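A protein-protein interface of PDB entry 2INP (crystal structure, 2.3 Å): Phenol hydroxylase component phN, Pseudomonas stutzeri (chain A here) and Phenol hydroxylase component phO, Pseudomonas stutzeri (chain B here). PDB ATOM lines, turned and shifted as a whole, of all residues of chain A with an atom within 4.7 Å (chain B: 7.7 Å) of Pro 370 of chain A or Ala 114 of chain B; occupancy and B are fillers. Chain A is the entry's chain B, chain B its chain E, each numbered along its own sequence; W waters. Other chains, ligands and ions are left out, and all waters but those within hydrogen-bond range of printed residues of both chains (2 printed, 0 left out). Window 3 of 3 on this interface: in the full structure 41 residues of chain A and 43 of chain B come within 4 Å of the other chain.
Among the printed residues, merely in contact across the chains: Tyr 374 of chain A with Met 113 of chain B (3.1 Å), Arg 371 of chain A with Tyr 118 of chain B (3.2 Å), Lys 366 of chain A with Ala 116 of chain B (3.5 Å), Pro 370 of chain A with Ala 114 of chain B (3.7 Å) and Tyr 374 of chain A with Tyr 118 of chain B (3.9 Å).
Water W2 bridges O of Ala 114 of chain B and O of Lys 366 of chain A.
Water W1 lies within hydrogen-bond range of the guanidinium group (NH2) of Arg 371 of chain A, the backbone carbonyl oxygen (O) of Tyr 367 of chain A and the backbone carbonyl oxygen (O) of Ala 116 of chain B.
The backbone NH of Met 113 of chain B sits at hydrogen-bond distance from the chain-end carboxylate of Tyr 118 of chain B (2.8 Å).
Arg 369 of chain A touches none of the printed residues of chain B.
Of the printed residues of chain B, Arg 371 of chain A touches Tyr 118 (3.2 Å).
Ala 114 of chain B touches one residue of chain A.
Of the printed residues of chain A, Tyr 118 of chain B touches Arg 371 and Tyr 374.
The nearest residue of chain B that does not touch Pro 370 of chain A is Ala 116 of chain B (4.6 Å).
The nearest residue of chain A that does not touch Ala 114 of chain B is Lys 366 of chain A (4.4 Å).
Printed residues of chain A that touch a printed residue of chain B: Lys 366, Pro 370, Arg 371 and Tyr 374.
Hydrophobic or aromatic side chains of chain B that line the printed part of chain A: Met 113, Ala 114, Ala 116 and Tyr 118.
Among the printed residues, no Asp or Glu carboxylate lies within 4 Å of a Lys or Arg side-chain nitrogen of the other chain.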
ATOM      1  N   PHE A 364      -0.065   2.513  30.382  1.00  0.00           N
ATOM      2  CA  PHE A 364      -0.783   3.426  31.264  1.00  0.00           C
ATOM      3  C   PHE A 364      -0.922   4.871  30.740  1.00  0.00           C
ATOM      4  O   PHE A 364      -2.062   5.464  30.662  1.00  0.00           O
ATOM      5  CB  PHE A 364      -0.280   3.358  32.723  1.00  0.00           C
ATOM      6  CG  PHE A 364      -1.178   4.064  33.679  1.00  0.00           C
ATOM      7  CD1 PHE A 364      -2.371   3.445  34.131  1.00  0.00           C
ATOM      8  CD2 PHE A 364      -0.896   5.367  34.086  1.00  0.00           C
ATOM      9  CE1 PHE A 364      -3.212   4.081  34.959  1.00  0.00           C
ATOM     10  CE2 PHE A 364      -1.736   6.024  34.943  1.00  0.00           C
ATOM     11  CZ  PHE A 364      -2.901   5.384  35.391  1.00  0.00           C
ATOM     12  N   ASP A 365       0.237   5.457  30.429  1.00  0.00           N
ATOM     13  CA  ASP A 365       0.314   6.845  30.019  1.00  0.00           C
ATOM     14  C   ASP A 365      -0.319   7.060  28.652  1.00  0.00           C
ATOM     15  O   ASP A 365      -0.979   8.064  28.426  1.00  0.00           O
ATOM     16  CB  ASP A 365       1.762   7.279  30.007  1.00  0.00           C
ATOM     17  CG  ASP A 365       2.327   7.465  31.389  1.00  0.00           C
ATOM     18  OD1 ASP A 365       1.639   7.325  32.421  1.00  0.00           O
ATOM     19  OD2 ASP A 365       3.499   7.813  31.438  1.00  0.00           O
ATOM     20  N   LYS A 366      -0.110   6.112  27.752  1.00  0.00           N
ATOM     21  CA  LYS A 366      -0.735   6.173  26.432  1.00  0.00           C
ATOM     22  C   LYS A 366      -2.300   6.174  26.567  1.00  0.00           C
ATOM     23  O   LYS A 366      -2.993   7.104  26.088  1.00  0.00           O
ATOM     24  CB  LYS A 366      -0.246   4.998  25.539  1.00  0.00           C
ATOM     25  CG  LYS A 366      -0.522   5.219  24.059  1.00  0.00           C
ATOM     26  CD  LYS A 366       0.147   4.149  23.149  1.00  0.00           C
ATOM     27  CE  LYS A 366       1.532   4.588  22.707  1.00  0.00           C
ATOM     28  NZ  LYS A 366       2.524   3.441  22.531  1.00  0.00           N
ATOM     29  N   TYR A 367      -2.824   5.190  27.296  1.00  0.00           N
ATOM     30  CA  TYR A 367      -4.255   4.846  27.252  1.00  0.00           C
ATOM     31  C   TYR A 367      -5.092   5.279  28.441  1.00  0.00           C
ATOM     32  O   TYR A 367      -6.225   5.676  28.234  1.00  0.00           O
ATOM     33  CB  TYR A 367      -4.439   3.350  27.000  1.00  0.00           C
ATOM     34  CG  TYR A 367      -3.836   2.869  25.707  1.00  0.00           C
ATOM     35  CD1 TYR A 367      -2.741   2.019  25.704  1.00  0.00           C
ATOM     36  CD2 TYR A 367      -4.374   3.279  24.478  1.00  0.00           C
ATOM     37  CE1 TYR A 367      -2.203   1.547  24.517  1.00  0.00           C
ATOM     38  CE2 TYR A 367      -3.852   2.840  23.286  1.00  0.00           C
ATOM     39  CZ  TYR A 367      -2.758   1.976  23.304  1.00  0.00           C
ATOM     40  OH  TYR A 367      -2.251   1.539  22.088  1.00  0.00           O
ATOM     41  N   TYR A 368      -4.535   5.233  29.660  1.00  0.00           N
ATOM     42  CA  TYR A 368      -5.321   5.337  30.906  1.00  0.00           C
ATOM     43  C   TYR A 368      -5.103   6.619  31.711  1.00  0.00           C
ATOM     44  O   TYR A 368      -6.060   7.213  32.208  1.00  0.00           O
ATOM     45  CB  TYR A 368      -5.229   4.022  31.720  1.00  0.00           C
ATOM     46  CG  TYR A 368      -5.545   2.850  30.824  1.00  0.00           C
ATOM     47  CD1 TYR A 368      -4.549   1.944  30.413  1.00  0.00           C
ATOM     48  CD2 TYR A 368      -6.863   2.669  30.299  1.00  0.00           C
ATOM     49  CE1 TYR A 368      -4.836   0.904  29.533  1.00  0.00           C
ATOM     50  CE2 TYR A 368      -7.149   1.632  29.450  1.00  0.00           C
ATOM     51  CZ  TYR A 368      -6.163   0.768  29.050  1.00  0.00           C
ATOM     52  OH  TYR A 368      -6.518  -0.264  28.185  1.00  0.00           O
ATOM     53  N   ARG A 369      -3.879   7.114  31.797  1.00  0.00           N
ATOM     54  CA  ARG A 369      -3.654   8.363  32.528  1.00  0.00           C
ATOM     55  C   ARG A 369      -4.503   9.515  31.989  1.00  0.00           C
ATOM     56  O   ARG A 369      -5.017  10.315  32.778  1.00  0.00           O
ATOM     57  CB  ARG A 369      -2.167   8.753  32.582  1.00  0.00           C
ATOM     58  CG  ARG A 369      -1.899  10.086  33.245  1.00  0.00           C
ATOM     59  CD  ARG A 369      -0.412  10.475  33.265  1.00  0.00           C
ATOM     60  NE  ARG A 369       0.377   9.573  34.104  1.00  0.00           N
ATOM     61  CZ  ARG A 369       0.682   9.792  35.373  1.00  0.00           C
ATOM     62  NH1 ARG A 369       0.249  10.892  35.996  1.00  0.00           N
ATOM     63  NH2 ARG A 369       1.395   8.869  36.018  1.00  0.00           N
ATOM     64  N   PRO A 370      -4.616   9.649  30.650  1.00  0.00           N
ATOM     65  CA  PRO A 370      -5.507  10.705  30.105  1.00  0.00           C
ATOM     66  C   PRO A 370      -6.979  10.566  30.544  1.00  0.00           C
ATOM     67  O   PRO A 370      -7.660  11.592  30.752  1.00  0.00           O
ATOM     68  CB  PRO A 370      -5.347  10.589  28.573  1.00  0.00           C
ATOM     69  CG  PRO A 370      -4.267   9.712  28.311  1.00  0.00           C
ATOM     70  CD  PRO A 370      -3.875   8.959  29.584  1.00  0.00           C
ATOM     71  N   ARG A 371      -7.453   9.342  30.790  1.00  0.00           N
ATOM     72  CA  ARG A 371      -8.800   9.200  31.343  1.00  0.00           C
ATOM     73  C   ARG A 371      -8.876   9.947  32.661  1.00  0.00           C
ATOM     74  O   ARG A 371      -9.734  10.840  32.800  1.00  0.00           O
ATOM     75  CB  ARG A 371      -9.203   7.738  31.484  1.00  0.00           C
ATOM     76  CG  ARG A 371      -8.994   6.921  30.199  1.00  0.00           C
ATOM     77  CD  ARG A 371      -9.646   5.600  30.344  1.00  0.00           C
ATOM     78  NE  ARG A 371      -9.565   4.854  29.088  1.00  0.00           N
ATOM     79  CZ  ARG A 371     -10.112   3.670  28.859  1.00  0.00           C
ATOM     80  NH1 ARG A 371     -10.813   3.053  29.812  1.00  0.00           N
ATOM     81  NH2 ARG A 371      -9.932   3.079  27.684  1.00  0.00           N
ATOM     82  N   TYR A 372      -7.961   9.653  33.592  1.00  0.00           N
ATOM     83  CA  TYR A 372      -8.011  10.245  34.941  1.00  0.00           C
ATOM     84  C   TYR A 372      -7.863  11.731  34.965  1.00  0.00           C
ATOM     85  O   TYR A 372      -8.524  12.391  35.790  1.00  0.00           O
ATOM     86  CB  TYR A 372      -7.027   9.540  35.926  1.00  0.00           C
ATOM     87  CG  TYR A 372      -7.319   8.090  35.947  1.00  0.00           C
ATOM     88  CD1 TYR A 372      -8.606   7.628  36.314  1.00  0.00           C
ATOM     89  CD2 TYR A 372      -6.392   7.166  35.537  1.00  0.00           C
ATOM     90  CE1 TYR A 372      -8.933   6.288  36.280  1.00  0.00           C
ATOM     91  CE2 TYR A 372      -6.736   5.812  35.479  1.00  0.00           C
ATOM     92  CZ  TYR A 372      -8.019   5.387  35.845  1.00  0.00           C
ATOM     93  OH  TYR A 372      -8.365   4.028  35.825  1.00  0.00           O
ATOM     94  N   GLU A 373      -7.034  12.263  34.048  1.00  0.00           N
ATOM     95  CA  GLU A 373      -6.871  13.714  33.813  1.00  0.00           C
ATOM     96  C   GLU A 373      -8.192  14.395  33.350  1.00  0.00           C
ATOM     97  O   GLU A 373      -8.655  15.450  33.911  1.00  0.00           O
ATOM     98  CB  GLU A 373      -5.779  13.942  32.777  1.00  0.00           C
ATOM     99  CG  GLU A 373      -4.318  13.812  33.299  1.00  0.00           C
ATOM    100  CD  GLU A 373      -3.245  13.601  32.141  1.00  0.00           C
ATOM    101  OE1 GLU A 373      -2.101  13.156  32.460  1.00  0.00           O
ATOM    102  OE2 GLU A 373      -3.523  13.851  30.924  1.00  0.00           O
ATOM    103  N   TYR A 374      -8.823  13.747  32.373  1.00  0.00           N
ATOM    104  CA  TYR A 374     -10.128  14.175  31.877  1.00  0.00           C
ATOM    105  C   TYR A 374     -11.192  14.094  32.990  1.00  0.00           C
ATOM    106  O   TYR A 374     -11.853  15.100  33.354  1.00  0.00           O
ATOM    107  CB  TYR A 374     -10.530  13.360  30.621  1.00  0.00           C
ATOM    108  CG  TYR A 374     -11.916  13.792  30.175  1.00  0.00           C
ATOM    109  CD1 TYR A 374     -12.108  14.994  29.455  1.00  0.00           C
ATOM    110  CD2 TYR A 374     -13.038  13.054  30.543  1.00  0.00           C
ATOM    111  CE1 TYR A 374     -13.375  15.426  29.110  1.00  0.00           C
ATOM    112  CE2 TYR A 374     -14.306  13.459  30.203  1.00  0.00           C
ATOM    113  CZ  TYR A 374     -14.470  14.617  29.462  1.00  0.00           C
ATOM    114  OH  TYR A 374     -15.724  14.989  29.143  1.00  0.00           O
ATOM    115  N   LYS B 111     -12.176  11.322  16.711  1.00  0.00           N
ATOM    116  CA  LYS B 111     -11.656  10.060  17.236  1.00  0.00           C
ATOM    117  C   LYS B 111     -11.283  10.063  18.728  1.00  0.00           C
ATOM    118  O   LYS B 111     -10.388   9.354  19.176  1.00  0.00           O
ATOM    119  CB  LYS B 111     -10.667   9.318  16.283  1.00  0.00           C
ATOM    120  CG  LYS B 111      -9.674  10.158  15.531  1.00  0.00           C
ATOM    121  CD  LYS B 111      -9.685   9.920  13.976  1.00  0.00           C
ATOM    122  CE  LYS B 111      -9.807   8.459  13.490  1.00  0.00           C
ATOM    123  NZ  LYS B 111      -8.719   7.532  13.960  1.00  0.00           N
ATOM    124  N   GLY B 112     -12.024  10.838  19.503  1.00  0.00           N
ATOM    125  CA  GLY B 112     -11.842  10.778  20.928  1.00  0.00           C
ATOM    126  C   GLY B 112     -10.658  11.616  21.305  1.00  0.00           C
ATOM    127  O   GLY B 112     -10.031  12.293  20.445  1.00  0.00           O
ATOM    128  N   MET B 113     -10.375  11.601  22.594  1.00  0.00           N
ATOM    129  CA  MET B 113      -9.342  12.437  23.195  1.00  0.00           C
ATOM    130  C   MET B 113      -7.956  11.792  23.307  1.00  0.00           C
ATOM    131  O   MET B 113      -7.819  10.552  23.350  1.00  0.00           O
ATOM    132  CB  MET B 113      -9.771  12.922  24.586  1.00  0.00           C
ATOM    133  CG  MET B 113     -11.240  13.260  24.761  1.00  0.00           C
ATOM    134  SD  MET B 113     -11.508  13.511  26.567  1.00  0.00           S
ATOM    135  CE  MET B 113     -11.224  15.336  26.543  1.00  0.00           C
ATOM    136  N   ALA B 114      -6.953  12.692  23.320  1.00  0.00           N
ATOM    137  CA  ALA B 114      -5.592  12.410  23.743  1.00  0.00           C
ATOM    138  C   ALA B 114      -4.985  11.262  22.942  1.00  0.00           C
ATOM    139  O   ALA B 114      -4.237  10.452  23.491  1.00  0.00           O
ATOM    140  CB  ALA B 114      -5.587  12.081  25.213  1.00  0.00           C
ATOM    141  N   ASN B 115      -5.346  11.144  21.673  1.00  0.00           N
ATOM    142  CA  ASN B 115      -4.886  10.014  20.824  1.00  0.00           C
ATOM    143  C   ASN B 115      -5.069   8.620  21.365  1.00  0.00           C
ATOM    144  O   ASN B 115      -4.467   7.670  20.839  1.00  0.00           O
ATOM    145  CB  ASN B 115      -3.435  10.223  20.293  1.00  0.00           C
ATOM    146  CG  ASN B 115      -3.333  11.485  19.454  1.00  0.00           C
ATOM    147  OD1 ASN B 115      -3.894  11.541  18.365  1.00  0.00           O
ATOM    148  ND2 ASN B 115      -2.710  12.528  19.994  1.00  0.00           N
ATOM    149  N   ALA B 116      -5.981   8.516  22.349  1.00  0.00           N
ATOM    150  CA  ALA B 116      -6.265   7.282  23.110  1.00  0.00           C
ATOM    151  C   ALA B 116      -7.680   6.691  22.792  1.00  0.00           C
ATOM    152  O   ALA B 116      -8.103   5.718  23.411  1.00  0.00           O
ATOM    153  CB  ALA B 116      -6.096   7.569  24.617  1.00  0.00           C
ATOM    154  N   GLY B 117      -8.396   7.289  21.825  1.00  0.00           N
ATOM    155  CA  GLY B 117      -9.721   6.809  21.433  1.00  0.00           C
ATOM    156  C   GLY B 117     -10.722   6.900  22.596  1.00  0.00           C
ATOM    157  O   GLY B 117     -11.609   6.089  22.722  1.00  0.00           O
ATOM    158  N   TYR B 118     -10.547   7.895  23.445  1.00  0.00           N
ATOM    159  CA  TYR B 118     -11.268   7.995  24.685  1.00  0.00           C
ATOM    160  C   TYR B 118     -12.401   9.034  24.550  1.00  0.00           C
ATOM    161  O   TYR B 118     -13.526   8.667  24.920  1.00  0.00           O
ATOM    162  CB  TYR B 118     -10.332   8.368  25.875  1.00  0.00           C
ATOM    163  CG  TYR B 118     -11.043   8.378  27.232  1.00  0.00           C
ATOM    164  CD1 TYR B 118     -11.561   7.190  27.767  1.00  0.00           C
ATOM    165  CD2 TYR B 118     -11.153   9.563  28.002  1.00  0.00           C
ATOM    166  CE1 TYR B 118     -12.168   7.150  29.039  1.00  0.00           C
ATOM    167  CE2 TYR B 118     -11.828   9.557  29.298  1.00  0.00           C
ATOM    168  CZ  TYR B 118     -12.323   8.308  29.761  1.00  0.00           C
ATOM    169  OH  TYR B 118     -12.913   8.189  30.943  1.00  0.00           O
ATOM    170  OXT TYR B 118     -12.236  10.186  24.138  1.00  0.00           O
HETATM  171  O   HOH W   1      -8.228   4.805  26.333  1.00  0.00           O
HETATM  172  O   HOH W   2      -2.348   9.190  24.540  1.00  0.00           O
